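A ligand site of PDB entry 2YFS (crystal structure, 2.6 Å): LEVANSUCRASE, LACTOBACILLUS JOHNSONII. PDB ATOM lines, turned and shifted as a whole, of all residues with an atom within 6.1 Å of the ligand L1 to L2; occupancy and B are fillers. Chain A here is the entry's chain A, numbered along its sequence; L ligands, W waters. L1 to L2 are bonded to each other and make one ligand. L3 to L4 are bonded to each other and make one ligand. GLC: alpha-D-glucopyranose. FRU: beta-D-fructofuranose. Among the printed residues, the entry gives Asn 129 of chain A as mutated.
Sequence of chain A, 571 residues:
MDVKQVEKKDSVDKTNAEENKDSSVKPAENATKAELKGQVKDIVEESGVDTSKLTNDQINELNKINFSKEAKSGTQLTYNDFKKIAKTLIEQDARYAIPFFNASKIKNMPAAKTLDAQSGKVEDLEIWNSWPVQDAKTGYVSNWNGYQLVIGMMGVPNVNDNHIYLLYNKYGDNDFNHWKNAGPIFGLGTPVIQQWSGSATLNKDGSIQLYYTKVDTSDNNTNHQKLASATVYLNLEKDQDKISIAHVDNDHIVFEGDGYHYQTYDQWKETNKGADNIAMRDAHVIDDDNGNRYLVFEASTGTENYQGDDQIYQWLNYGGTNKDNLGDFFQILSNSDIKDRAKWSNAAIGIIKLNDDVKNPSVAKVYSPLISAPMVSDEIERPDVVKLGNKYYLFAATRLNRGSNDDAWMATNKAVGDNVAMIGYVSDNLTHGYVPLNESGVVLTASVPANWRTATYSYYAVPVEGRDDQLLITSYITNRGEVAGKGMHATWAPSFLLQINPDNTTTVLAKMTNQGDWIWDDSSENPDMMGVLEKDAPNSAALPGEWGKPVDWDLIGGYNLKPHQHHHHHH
The side-chain carboxylate (OE1) of Glu 379 sits at hydrogen-bond distance from an oxygen (O3) of GLC L1, 2.6 Å away.
OD1 of Asp 282 lies within hydrogen-bond range of O4 of FRU L2, 2.6 Å away.
O1 of FRU L2 lies within hydrogen-bond range of ND2 of Asn 129 (2.7 Å).
NH2 of Arg 399 sits at hydrogen-bond distance from O2 of GLC L1.
An oxygen (O6) of FRU L2 is in hydrogen-bond range of the indole nitrogen of Trp 128 (3.0 Å).
An oxygen (O3) of FRU L2 sits at hydrogen-bond distance from the side-chain carboxylate of Glu 381, at 3.1 Å.
The backbone NH (N) of Ser 197 lies within hydrogen-bond range of an oxygen (O4) of FRU L2.
O4 of FRU L2 lies within hydrogen-bond range of OG of Ser 197 (3.2 Å).
O3 of FRU L2 lies within hydrogen-bond range of NE of Arg 281 (3.2 Å).
An oxygen (O6) of FRU L2 lies close to the side-chain sulfur of Met 153 (3.5 Å).
The guanidinium group (NH2) of Arg 480 is in hydrogen-bond range of an oxygen (O3) of FRU L4 (2.8 Å).
An oxygen (O4) of FRU L4 lies within hydrogen-bond range of the side-chain amide nitrogen (ND2) of Asn 162 (3.5 Å).
The side-chain carboxylate (OE1) of Glu 379 is in salt-bridge range of the guanidinium group (NE) of Arg 402.
The backbone NH of Asp 282 lies within hydrogen-bond range of the backbone carbonyl oxygen of Ser 197, at 3.4 Å.
The backbone carbonyl oxygen (O) of Asn 129 is in hydrogen-bond range of the backbone NH (N) of Met 153 (2.9 Å).
The guanidinium group (NE) of Arg 399 lies within salt-bridge range of the side-chain carboxylate (OE2) of Glu 381, 3.95 Å away.
OE1 of Glu 381 is in salt-bridge range of NH2 of Arg 281.
The side-chain carboxylate (OE2) of Glu 381 sits at hydrogen-bond distance from the side-chain hydroxyl (OH) of Tyr 457 (2.6 Å).
OG of Ser 197 lies within hydrogen-bond range of SD of Met 153.
The side-chain hydroxyl of Thr 213 lies within hydrogen-bond range of the backbone carbonyl oxygen of Ser 197.
CB of Trp 196 touches O4 of FRU L2, at 3.6 Å.
Glu 298 touches the ligand L1 to L2.
NE of Arg 402 touches O3 of GLC L1, 3.8 Å away.
CE2 of Tyr 457 touches C1 of FRU L2, 3.9 Å away.
OG of Ser 458 touches O1 of FRU L2, 3.6 Å away.
Arg 480 touches the ligand L1 to L2.
Along chain A the residues within 4 Å of the ligand L1 to L2 span positions 128 to 480.
Water W1 lies within hydrogen-bond range of O6 of FRU L2 (2.8 Å), NH1 of Arg 480 (2.8 Å) and OD1 of Asn 162 (2.9 Å).
Water W3 lies within hydrogen-bond range of NH1 of Arg 480 (2.8 Å) and O6 of FRU L2 (3.1 Å).
Water W2 lies within hydrogen-bond range of OH of Tyr 476 (2.9 Å) and O1 of FRU L2 (3.1 Å).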
ATOM      1  N   TRP A 128      27.640 -24.324  19.812  1.00  0.00           N
ATOM      2  CA  TRP A 128      26.935 -25.607  19.934  1.00  0.00           C
ATOM      3  C   TRP A 128      25.599 -25.688  19.197  1.00  0.00           C
ATOM      4  O   TRP A 128      25.610 -25.619  17.976  1.00  0.00           O
ATOM      5  CB  TRP A 128      26.870 -26.104  21.378  1.00  0.00           C
ATOM      6  CG  TRP A 128      26.324 -25.188  22.410  1.00  0.00           C
ATOM      7  CD1 TRP A 128      25.125 -25.302  23.055  1.00  0.00           C
ATOM      8  CD2 TRP A 128      26.966 -24.028  22.969  1.00  0.00           C
ATOM      9  NE1 TRP A 128      24.985 -24.293  23.977  1.00  0.00           N
ATOM     10  CE2 TRP A 128      26.096 -23.506  23.955  1.00  0.00           C
ATOM     11  CE3 TRP A 128      28.198 -23.396  22.749  1.00  0.00           C
ATOM     12  CZ2 TRP A 128      26.405 -22.366  24.715  1.00  0.00           C
ATOM     13  CZ3 TRP A 128      28.512 -22.263  23.520  1.00  0.00           C
ATOM     14  CH2 TRP A 128      27.619 -21.762  24.486  1.00  0.00           C
ATOM     15  N   ASN A 129      24.491 -25.869  19.911  1.00  0.00           N
ATOM     16  CA  ASN A 129      23.199 -26.046  19.249  1.00  0.00           C
ATOM     17  C   ASN A 129      23.001 -25.018  18.135  1.00  0.00           C
ATOM     18  O   ASN A 129      23.154 -23.849  18.361  1.00  0.00           O
ATOM     19  CB  ASN A 129      22.043 -25.923  20.216  1.00  0.00           C
ATOM     20  CG  ASN A 129      22.081 -26.961  21.311  1.00  0.00           C
ATOM     21  OD1 ASN A 129      23.103 -27.613  21.533  1.00  0.00           O
ATOM     22  ND2 ASN A 129      20.962 -27.106  22.047  1.00  0.00           N
ATOM     23  N   MET A 153      23.874 -21.184  19.309  1.00  0.00           N
ATOM     24  CA  MET A 153      24.343 -20.802  20.611  1.00  0.00           C
ATOM     25  C   MET A 153      25.860 -20.728  20.600  1.00  0.00           C
ATOM     26  O   MET A 153      26.513 -21.646  20.125  1.00  0.00           O
ATOM     27  CB  MET A 153      23.837 -21.776  21.653  1.00  0.00           C
ATOM     28  CG  MET A 153      22.354 -21.654  21.884  1.00  0.00           C
ATOM     29  SD  MET A 153      21.756 -22.704  23.225  1.00  0.00           S
ATOM     30  CE  MET A 153      22.495 -21.870  24.639  1.00  0.00           C
ATOM     31  N   ASN A 162      25.418 -17.902  27.536  1.00  0.00           N
ATOM     32  CA  ASN A 162      24.475 -18.543  26.602  1.00  0.00           C
ATOM     33  C   ASN A 162      23.635 -17.549  25.775  1.00  0.00           C
ATOM     34  O   ASN A 162      22.595 -17.055  26.226  1.00  0.00           O
ATOM     35  CB  ASN A 162      23.542 -19.476  27.373  1.00  0.00           C
ATOM     36  CG  ASN A 162      24.290 -20.479  28.200  1.00  0.00           C
ATOM     37  OD1 ASN A 162      25.101 -21.228  27.672  1.00  0.00           O
ATOM     38  ND2 ASN A 162      24.039 -20.497  29.494  1.00  0.00           N
ATOM     39  N   TRP A 196      18.417 -19.698  24.497  1.00  0.00           N
ATOM     40  CA  TRP A 196      18.745 -21.057  24.153  1.00  0.00           C
ATOM     41  C   TRP A 196      18.030 -21.423  22.839  1.00  0.00           C
ATOM     42  O   TRP A 196      17.418 -20.578  22.208  1.00  0.00           O
ATOM     43  CB  TRP A 196      18.326 -21.999  25.274  1.00  0.00           C
ATOM     44  CG  TRP A 196      18.987 -21.739  26.599  1.00  0.00           C
ATOM     45  CD1 TRP A 196      19.855 -20.720  26.925  1.00  0.00           C
ATOM     46  CD2 TRP A 196      18.801 -22.498  27.809  1.00  0.00           C
ATOM     47  NE1 TRP A 196      20.238 -20.822  28.239  1.00  0.00           N
ATOM     48  CE2 TRP A 196      19.608 -21.892  28.802  1.00  0.00           C
ATOM     49  CE3 TRP A 196      18.038 -23.620  28.137  1.00  0.00           C
ATOM     50  CZ2 TRP A 196      19.673 -22.376  30.109  1.00  0.00           C
ATOM     51  CZ3 TRP A 196      18.098 -24.113  29.416  1.00  0.00           C
ATOM     52  CH2 TRP A 196      18.920 -23.485  30.399  1.00  0.00           C
ATOM     53  N   SER A 197      18.100 -22.685  22.440  1.00  0.00           N
ATOM     54  CA  SER A 197      17.725 -23.104  21.078  1.00  0.00           C
ATOM     55  C   SER A 197      16.278 -22.898  20.665  1.00  0.00           C
ATOM     56  O   SER A 197      15.381 -22.913  21.498  1.00  0.00           O
ATOM     57  CB  SER A 197      18.057 -24.567  20.894  1.00  0.00           C
ATOM     58  OG  SER A 197      19.392 -24.763  21.283  1.00  0.00           O
ATOM     59  N   THR A 213      14.451 -19.770  22.948  1.00  0.00           N
ATOM     60  CA  THR A 213      14.045 -19.914  24.334  1.00  0.00           C
ATOM     61  C   THR A 213      14.581 -18.753  25.138  1.00  0.00           C
ATOM     62  O   THR A 213      15.799 -18.625  25.297  1.00  0.00           O
ATOM     63  CB  THR A 213      14.638 -21.193  24.948  1.00  0.00           C
ATOM     64  OG1 THR A 213      14.324 -22.304  24.106  1.00  0.00           O
ATOM     65  CG2 THR A 213      14.142 -21.431  26.372  1.00  0.00           C
ATOM     66  N   ASN A 223      16.963 -21.607  35.875  1.00  0.00           N
ATOM     67  CA  ASN A 223      16.761 -21.380  34.442  1.00  0.00           C
ATOM     68  C   ASN A 223      15.279 -21.363  34.065  1.00  0.00           C
ATOM     69  O   ASN A 223      14.750 -22.329  33.539  1.00  0.00           O
ATOM     70  CB  ASN A 223      17.533 -22.410  33.617  1.00  0.00           C
ATOM     71  CG  ASN A 223      19.050 -22.331  33.817  1.00  0.00           C
ATOM     72  OD1 ASN A 223      19.659 -21.264  33.719  1.00  0.00           O
ATOM     73  ND2 ASN A 223      19.656 -23.486  34.058  1.00  0.00           N
ATOM     74  N   ASN A 277      14.204 -31.506  36.857  1.00  0.00           N
ATOM     75  CA  ASN A 277      14.522 -30.804  35.640  1.00  0.00           C
ATOM     76  C   ASN A 277      13.370 -29.865  35.330  1.00  0.00           C
ATOM     77  O   ASN A 277      12.217 -30.150  35.626  1.00  0.00           O
ATOM     78  CB  ASN A 277      14.734 -31.814  34.501  1.00  0.00           C
ATOM     79  CG  ASN A 277      15.194 -31.145  33.203  1.00  0.00           C
ATOM     80  OD1 ASN A 277      16.190 -30.414  33.190  1.00  0.00           O
ATOM     81  ND2 ASN A 277      14.461 -31.392  32.101  1.00  0.00           N
ATOM     82  N   ARG A 281      11.560 -25.380  26.222  1.00  0.00           N
ATOM     83  CA  ARG A 281      12.613 -24.933  25.328  1.00  0.00           C
ATOM     84  C   ARG A 281      12.653 -25.659  24.014  1.00  0.00           C
ATOM     85  O   ARG A 281      11.858 -26.555  23.763  1.00  0.00           O
ATOM     86  CB  ARG A 281      13.969 -25.051  26.018  1.00  0.00           C
ATOM     87  CG  ARG A 281      14.358 -26.449  26.444  1.00  0.00           C
ATOM     88  CD  ARG A 281      15.682 -26.425  27.138  1.00  0.00           C
ATOM     89  NE  ARG A 281      16.169 -27.768  27.452  1.00  0.00           N
ATOM     90  CZ  ARG A 281      16.261 -28.279  28.677  1.00  0.00           C
ATOM     91  NH1 ARG A 281      15.907 -27.558  29.733  1.00  0.00           N
ATOM     92  NH2 ARG A 281      16.705 -29.512  28.846  1.00  0.00           N
ATOM     93  N   ASP A 282      13.611 -25.263  23.165  1.00  0.00           N
ATOM     94  CA  ASP A 282      13.900 -25.946  21.917  1.00  0.00           C
ATOM     95  C   ASP A 282      12.703 -26.005  20.953  1.00  0.00           C
ATOM     96  O   ASP A 282      12.364 -27.079  20.456  1.00  0.00           O
ATOM     97  CB  ASP A 282      14.459 -27.362  22.176  1.00  0.00           C
ATOM     98  CG  ASP A 282      15.781 -27.351  22.939  1.00  0.00           C
ATOM     99  OD1 ASP A 282      16.365 -26.263  23.170  1.00  0.00           O
ATOM    100  OD2 ASP A 282      16.273 -28.446  23.301  1.00  0.00           O
ATOM    101  N   GLU A 298      10.534 -28.987  23.810  1.00  0.00           N
ATOM    102  CA  GLU A 298      10.826 -29.849  24.948  1.00  0.00           C
ATOM    103  C   GLU A 298      10.175 -29.284  26.219  1.00  0.00           C
ATOM    104  O   GLU A 298      10.261 -28.097  26.484  1.00  0.00           O
ATOM    105  CB  GLU A 298      12.348 -30.027  25.133  1.00  0.00           C
ATOM    106  CG  GLU A 298      12.794 -30.309  26.589  1.00  0.00           C
ATOM    107  CD  GLU A 298      14.304 -30.542  26.817  1.00  0.00           C
ATOM    108  OE1 GLU A 298      15.143 -30.029  26.028  1.00  0.00           O
ATOM    109  OE2 GLU A 298      14.650 -31.239  27.816  1.00  0.00           O
ATOM    110  N   GLU A 379      14.773 -35.901  30.441  1.00  0.00           N
ATOM    111  CA  GLU A 379      15.330 -35.042  29.405  1.00  0.00           C
ATOM    112  C   GLU A 379      15.369 -35.596  27.983  1.00  0.00           C
ATOM    113  O   GLU A 379      16.218 -36.422  27.644  1.00  0.00           O
ATOM    114  CB  GLU A 379      16.725 -34.542  29.804  1.00  0.00           C
ATOM    115  CG  GLU A 379      17.070 -33.201  29.146  1.00  0.00           C
ATOM    116  CD  GLU A 379      18.382 -32.620  29.600  1.00  0.00           C
ATOM    117  OE1 GLU A 379      19.451 -33.220  29.283  1.00  0.00           O
ATOM    118  OE2 GLU A 379      18.353 -31.543  30.254  1.00  0.00           O
ATOM    119  N   GLU A 381      15.467 -33.729  24.171  1.00  0.00           N
ATOM    120  CA  GLU A 381      15.823 -32.391  23.725  1.00  0.00           C
ATOM    121  C   GLU A 381      15.783 -32.178  22.222  1.00  0.00           C
ATOM    122  O   GLU A 381      15.756 -33.116  21.428  1.00  0.00           O
ATOM    123  CB  GLU A 381      17.227 -31.988  24.228  1.00  0.00           C
ATOM    124  CG  GLU A 381      17.770 -32.793  25.363  1.00  0.00           C
ATOM    125  CD  GLU A 381      18.865 -32.059  26.088  1.00  0.00           C
ATOM    126  OE1 GLU A 381      18.527 -31.071  26.788  1.00  0.00           O
ATOM    127  OE2 GLU A 381      20.048 -32.446  25.948  1.00  0.00           O
ATOM    128  N   ARG A 382      15.821 -30.919  21.832  1.00  0.00           N
ATOM    129  CA  ARG A 382      15.937 -30.547  20.429  1.00  0.00           C
ATOM    130  C   ARG A 382      15.070 -31.344  19.488  1.00  0.00           C
ATOM    131  O   ARG A 382      15.563 -31.943  18.568  1.00  0.00           O
ATOM    132  CB  ARG A 382      17.399 -30.594  19.987  1.00  0.00           C
ATOM    133  CG  ARG A 382      18.151 -29.349  20.455  1.00  0.00           C
ATOM    134  CD  ARG A 382      19.231 -28.978  19.494  1.00  0.00           C
ATOM    135  NE  ARG A 382      18.783 -28.119  18.398  1.00  0.00           N
ATOM    136  CZ  ARG A 382      19.539 -27.838  17.336  1.00  0.00           C
ATOM    137  NH1 ARG A 382      20.758 -28.361  17.212  1.00  0.00           N
ATOM    138  NH2 ARG A 382      19.087 -27.032  16.397  1.00  0.00           N
ATOM    139  N   ARG A 399      20.299 -37.693  26.353  1.00  0.00           N
ATOM    140  CA  ARG A 399      21.417 -38.188  27.104  1.00  0.00           C
ATOM    141  C   ARG A 399      20.883 -39.269  28.048  1.00  0.00           C
ATOM    142  O   ARG A 399      20.106 -38.977  28.972  1.00  0.00           O
ATOM    143  CB  ARG A 399      22.029 -37.065  27.938  1.00  0.00           C
ATOM    144  CG  ARG A 399      22.529 -35.852  27.194  1.00  0.00           C
ATOM    145  CD  ARG A 399      23.031 -34.811  28.204  1.00  0.00           C
ATOM    146  NE  ARG A 399      23.465 -33.566  27.592  1.00  0.00           N
ATOM    147  CZ  ARG A 399      24.608 -33.395  26.928  1.00  0.00           C
ATOM    148  NH1 ARG A 399      25.455 -34.421  26.749  1.00  0.00           N
ATOM    149  NH2 ARG A 399      24.904 -32.200  26.401  1.00  0.00           N
ATOM    150  N   ARG A 402      20.342 -39.059  31.900  1.00  0.00           N
ATOM    151  CA  ARG A 402      19.198 -38.346  32.494  1.00  0.00           C
ATOM    152  C   ARG A 402      18.045 -39.317  32.690  1.00  0.00           C
ATOM    153  O   ARG A 402      16.991 -38.956  33.209  1.00  0.00           O
ATOM    154  CB  ARG A 402      18.745 -37.160  31.626  1.00  0.00           C
ATOM    155  CG  ARG A 402      19.863 -36.329  30.990  1.00  0.00           C
ATOM    156  CD  ARG A 402      20.665 -35.514  32.014  1.00  0.00           C
ATOM    157  NE  ARG A 402      21.712 -34.675  31.390  1.00  0.00           N
ATOM    158  CZ  ARG A 402      22.986 -34.596  31.787  1.00  0.00           C
ATOM    159  NH1 ARG A 402      23.416 -35.292  32.834  1.00  0.00           N
ATOM    160  NH2 ARG A 402      23.847 -33.817  31.133  1.00  0.00           N
ATOM    161  N   TYR A 457      27.002 -34.204  19.816  1.00  0.00           N
ATOM    162  CA  TYR A 457      25.675 -34.107  20.409  1.00  0.00           C
ATOM    163  C   TYR A 457      24.810 -33.160  19.623  1.00  0.00           C
ATOM    164  O   TYR A 457      25.256 -32.579  18.633  1.00  0.00           O
ATOM    165  CB  TYR A 457      25.711 -33.730  21.894  1.00  0.00           C
ATOM    166  CG  TYR A 457      24.380 -33.950  22.610  1.00  0.00           C
ATOM    167  CD1 TYR A 457      23.726 -35.188  22.548  1.00  0.00           C
ATOM    168  CD2 TYR A 457      23.761 -32.924  23.332  1.00  0.00           C
ATOM    169  CE1 TYR A 457      22.500 -35.407  23.179  1.00  0.00           C
ATOM    170  CE2 TYR A 457      22.533 -33.107  23.984  1.00  0.00           C
ATOM    171  CZ  TYR A 457      21.895 -34.359  23.891  1.00  0.00           C
ATOM    172  OH  TYR A 457      20.688 -34.564  24.525  1.00  0.00           O
ATOM    173  N   SER A 458      23.543 -33.092  20.021  1.00  0.00           N
ATOM    174  CA  SER A 458      22.576 -32.139  19.499  1.00  0.00           C
ATOM    175  C   SER A 458      22.278 -32.359  18.025  1.00  0.00           C
ATOM    176  O   SER A 458      22.203 -31.406  17.232  1.00  0.00           O
ATOM    177  CB  SER A 458      23.067 -30.731  19.773  1.00  0.00           C
ATOM    178  OG  SER A 458      22.002 -29.819  19.754  1.00  0.00           O
ATOM    179  N   TYR A 476      26.897 -30.773  16.642  1.00  0.00           N
ATOM    180  CA  TYR A 476      28.133 -30.155  16.981  1.00  0.00           C
ATOM    181  C   TYR A 476      29.078 -31.219  17.468  1.00  0.00           C
ATOM    182  O   TYR A 476      28.636 -32.265  17.965  1.00  0.00           O
ATOM    183  CB  TYR A 476      27.957 -29.008  17.973  1.00  0.00           C
ATOM    184  CG  TYR A 476      27.639 -29.375  19.403  1.00  0.00           C
ATOM    185  CD1 TYR A 476      28.649 -29.632  20.334  1.00  0.00           C
ATOM    186  CD2 TYR A 476      26.306 -29.378  19.868  1.00  0.00           C
ATOM    187  CE1 TYR A 476      28.348 -29.913  21.637  1.00  0.00           C
ATOM    188  CE2 TYR A 476      26.007 -29.668  21.174  1.00  0.00           C
ATOM    189  CZ  TYR A 476      27.025 -29.941  22.044  1.00  0.00           C
ATOM    190  OH  TYR A 476      26.706 -30.237  23.345  1.00  0.00           O
ATOM    191  N   ARG A 480      31.375 -29.013  25.145  1.00  0.00           N
ATOM    192  CA  ARG A 480      31.670 -27.699  25.702  1.00  0.00           C
ATOM    193  C   ARG A 480      32.659 -27.792  26.863  1.00  0.00           C
ATOM    194  O   ARG A 480      33.003 -28.874  27.313  1.00  0.00           O
ATOM    195  CB  ARG A 480      30.358 -27.025  26.139  1.00  0.00           C
ATOM    196  CG  ARG A 480      29.390 -26.737  24.976  1.00  0.00           C
ATOM    197  CD  ARG A 480      28.042 -26.242  25.488  1.00  0.00           C
ATOM    198  NE  ARG A 480      28.236 -25.044  26.283  1.00  0.00           N
ATOM    199  CZ  ARG A 480      27.382 -24.564  27.183  1.00  0.00           C
ATOM    200  NH1 ARG A 480      26.235 -25.171  27.422  1.00  0.00           N
ATOM    201  NH2 ARG A 480      27.683 -23.452  27.846  1.00  0.00           N
HETATM  202  C1  GLC L   1      21.904 -28.407  27.440  1.00  0.00           C
HETATM  203  C2  GLC L   1      22.229 -29.739  28.156  1.00  0.00           C
HETATM  204  C3  GLC L   1      21.053 -30.092  29.034  1.00  0.00           C
HETATM  205  C4  GLC L   1      20.966 -29.049  30.148  1.00  0.00           C
HETATM  206  C5  GLC L   1      20.858 -27.631  29.565  1.00  0.00           C
HETATM  207  C6  GLC L   1      21.154 -26.677  30.739  1.00  0.00           C
HETATM  208  O2  GLC L   1      22.556 -30.849  27.294  1.00  0.00           O
HETATM  209  O3  GLC L   1      21.252 -31.400  29.553  1.00  0.00           O
HETATM  210  O4  GLC L   1      19.832 -29.327  30.994  1.00  0.00           O
HETATM  211  O5  GLC L   1      21.808 -27.393  28.458  1.00  0.00           O
HETATM  212  O6  GLC L   1      22.338 -25.890  30.468  1.00  0.00           O
HETATM  213  C1  FRU L   2      21.097 -29.548  24.663  1.00  0.00           C
HETATM  214  C2  FRU L   2      20.682 -28.197  25.283  1.00  0.00           C
HETATM  215  C3  FRU L   2      19.362 -27.706  24.679  1.00  0.00           C
HETATM  216  C4  FRU L   2      19.334 -26.240  25.165  1.00  0.00           C
HETATM  217  C5  FRU L   2      20.808 -25.867  25.002  1.00  0.00           C
HETATM  218  C6  FRU L   2      21.383 -24.982  26.123  1.00  0.00           C
HETATM  219  O1  FRU L   2      21.620 -29.369  23.349  1.00  0.00           O
HETATM  220  O2  FRU L   2      20.631 -28.357  26.744  1.00  0.00           O
HETATM  221  O3  FRU L   2      18.227 -28.466  25.125  1.00  0.00           O
HETATM  222  O4  FRU L   2      18.567 -25.431  24.266  1.00  0.00           O
HETATM  223  O5  FRU L   2      21.571 -27.103  24.939  1.00  0.00           O
HETATM  224  O6  FRU L   2      22.777 -24.805  25.889  1.00  0.00           O
HETATM  225  C1  GLC L   3      30.685 -25.423  32.666  1.00  0.00           C
HETATM  226  C2  GLC L   3      30.574 -26.394  31.471  1.00  0.00           C
HETATM  227  C3  GLC L   3      29.558 -27.487  31.807  1.00  0.00           C
HETATM  228  C4  GLC L   3      30.126 -28.267  33.014  1.00  0.00           C
HETATM  229  C5  GLC L   3      30.247 -27.292  34.216  1.00  0.00           C
HETATM  230  C6  GLC L   3      30.737 -27.982  35.506  1.00  0.00           C
HETATM  231  O2  GLC L   3      30.165 -25.720  30.288  1.00  0.00           O
HETATM  232  O3  GLC L   3      29.293 -28.307  30.669  1.00  0.00           O
HETATM  233  O4  GLC L   3      29.311 -29.416  33.329  1.00  0.00           O
HETATM  234  O5  GLC L   3      31.125 -26.139  33.866  1.00  0.00           O
HETATM  235  O6  GLC L   3      30.927 -27.000  36.521  1.00  0.00           O
HETATM  236  C1  FRU L   4      30.473 -22.593  32.899  1.00  0.00           C
HETATM  237  C2  FRU L   4      29.176 -23.392  32.834  1.00  0.00           C
HETATM  238  C3  FRU L   4      28.371 -23.056  31.559  1.00  0.00           C
HETATM  239  C4  FRU L   4      26.966 -23.405  32.021  1.00  0.00           C
HETATM  240  C5  FRU L   4      26.994 -22.629  33.348  1.00  0.00           C
HETATM  241  C6  FRU L   4      25.931 -22.895  34.443  1.00  0.00           C
HETATM  242  O1  FRU L   4      30.888 -22.430  34.262  1.00  0.00           O
HETATM  243  O2  FRU L   4      29.385 -24.850  32.961  1.00  0.00           O
HETATM  244  O3  FRU L   4      28.743 -23.865  30.442  1.00  0.00           O
HETATM  245  O4  FRU L   4      26.053 -22.852  31.083  1.00  0.00           O
HETATM  246  O5  FRU L   4      28.320 -22.934  33.923  1.00  0.00           O
HETATM  247  O6  FRU L   4      26.373 -22.304  35.684  1.00  0.00           O
HETATM  248  O   HOH W   1      23.889 -23.843  28.268  1.00  0.00           O
HETATM  249  O   HOH W   2      24.409 -29.152  24.655  1.00  0.00           O
HETATM  250  O   HOH W   3      24.629 -27.205  26.370  1.00  0.00           O
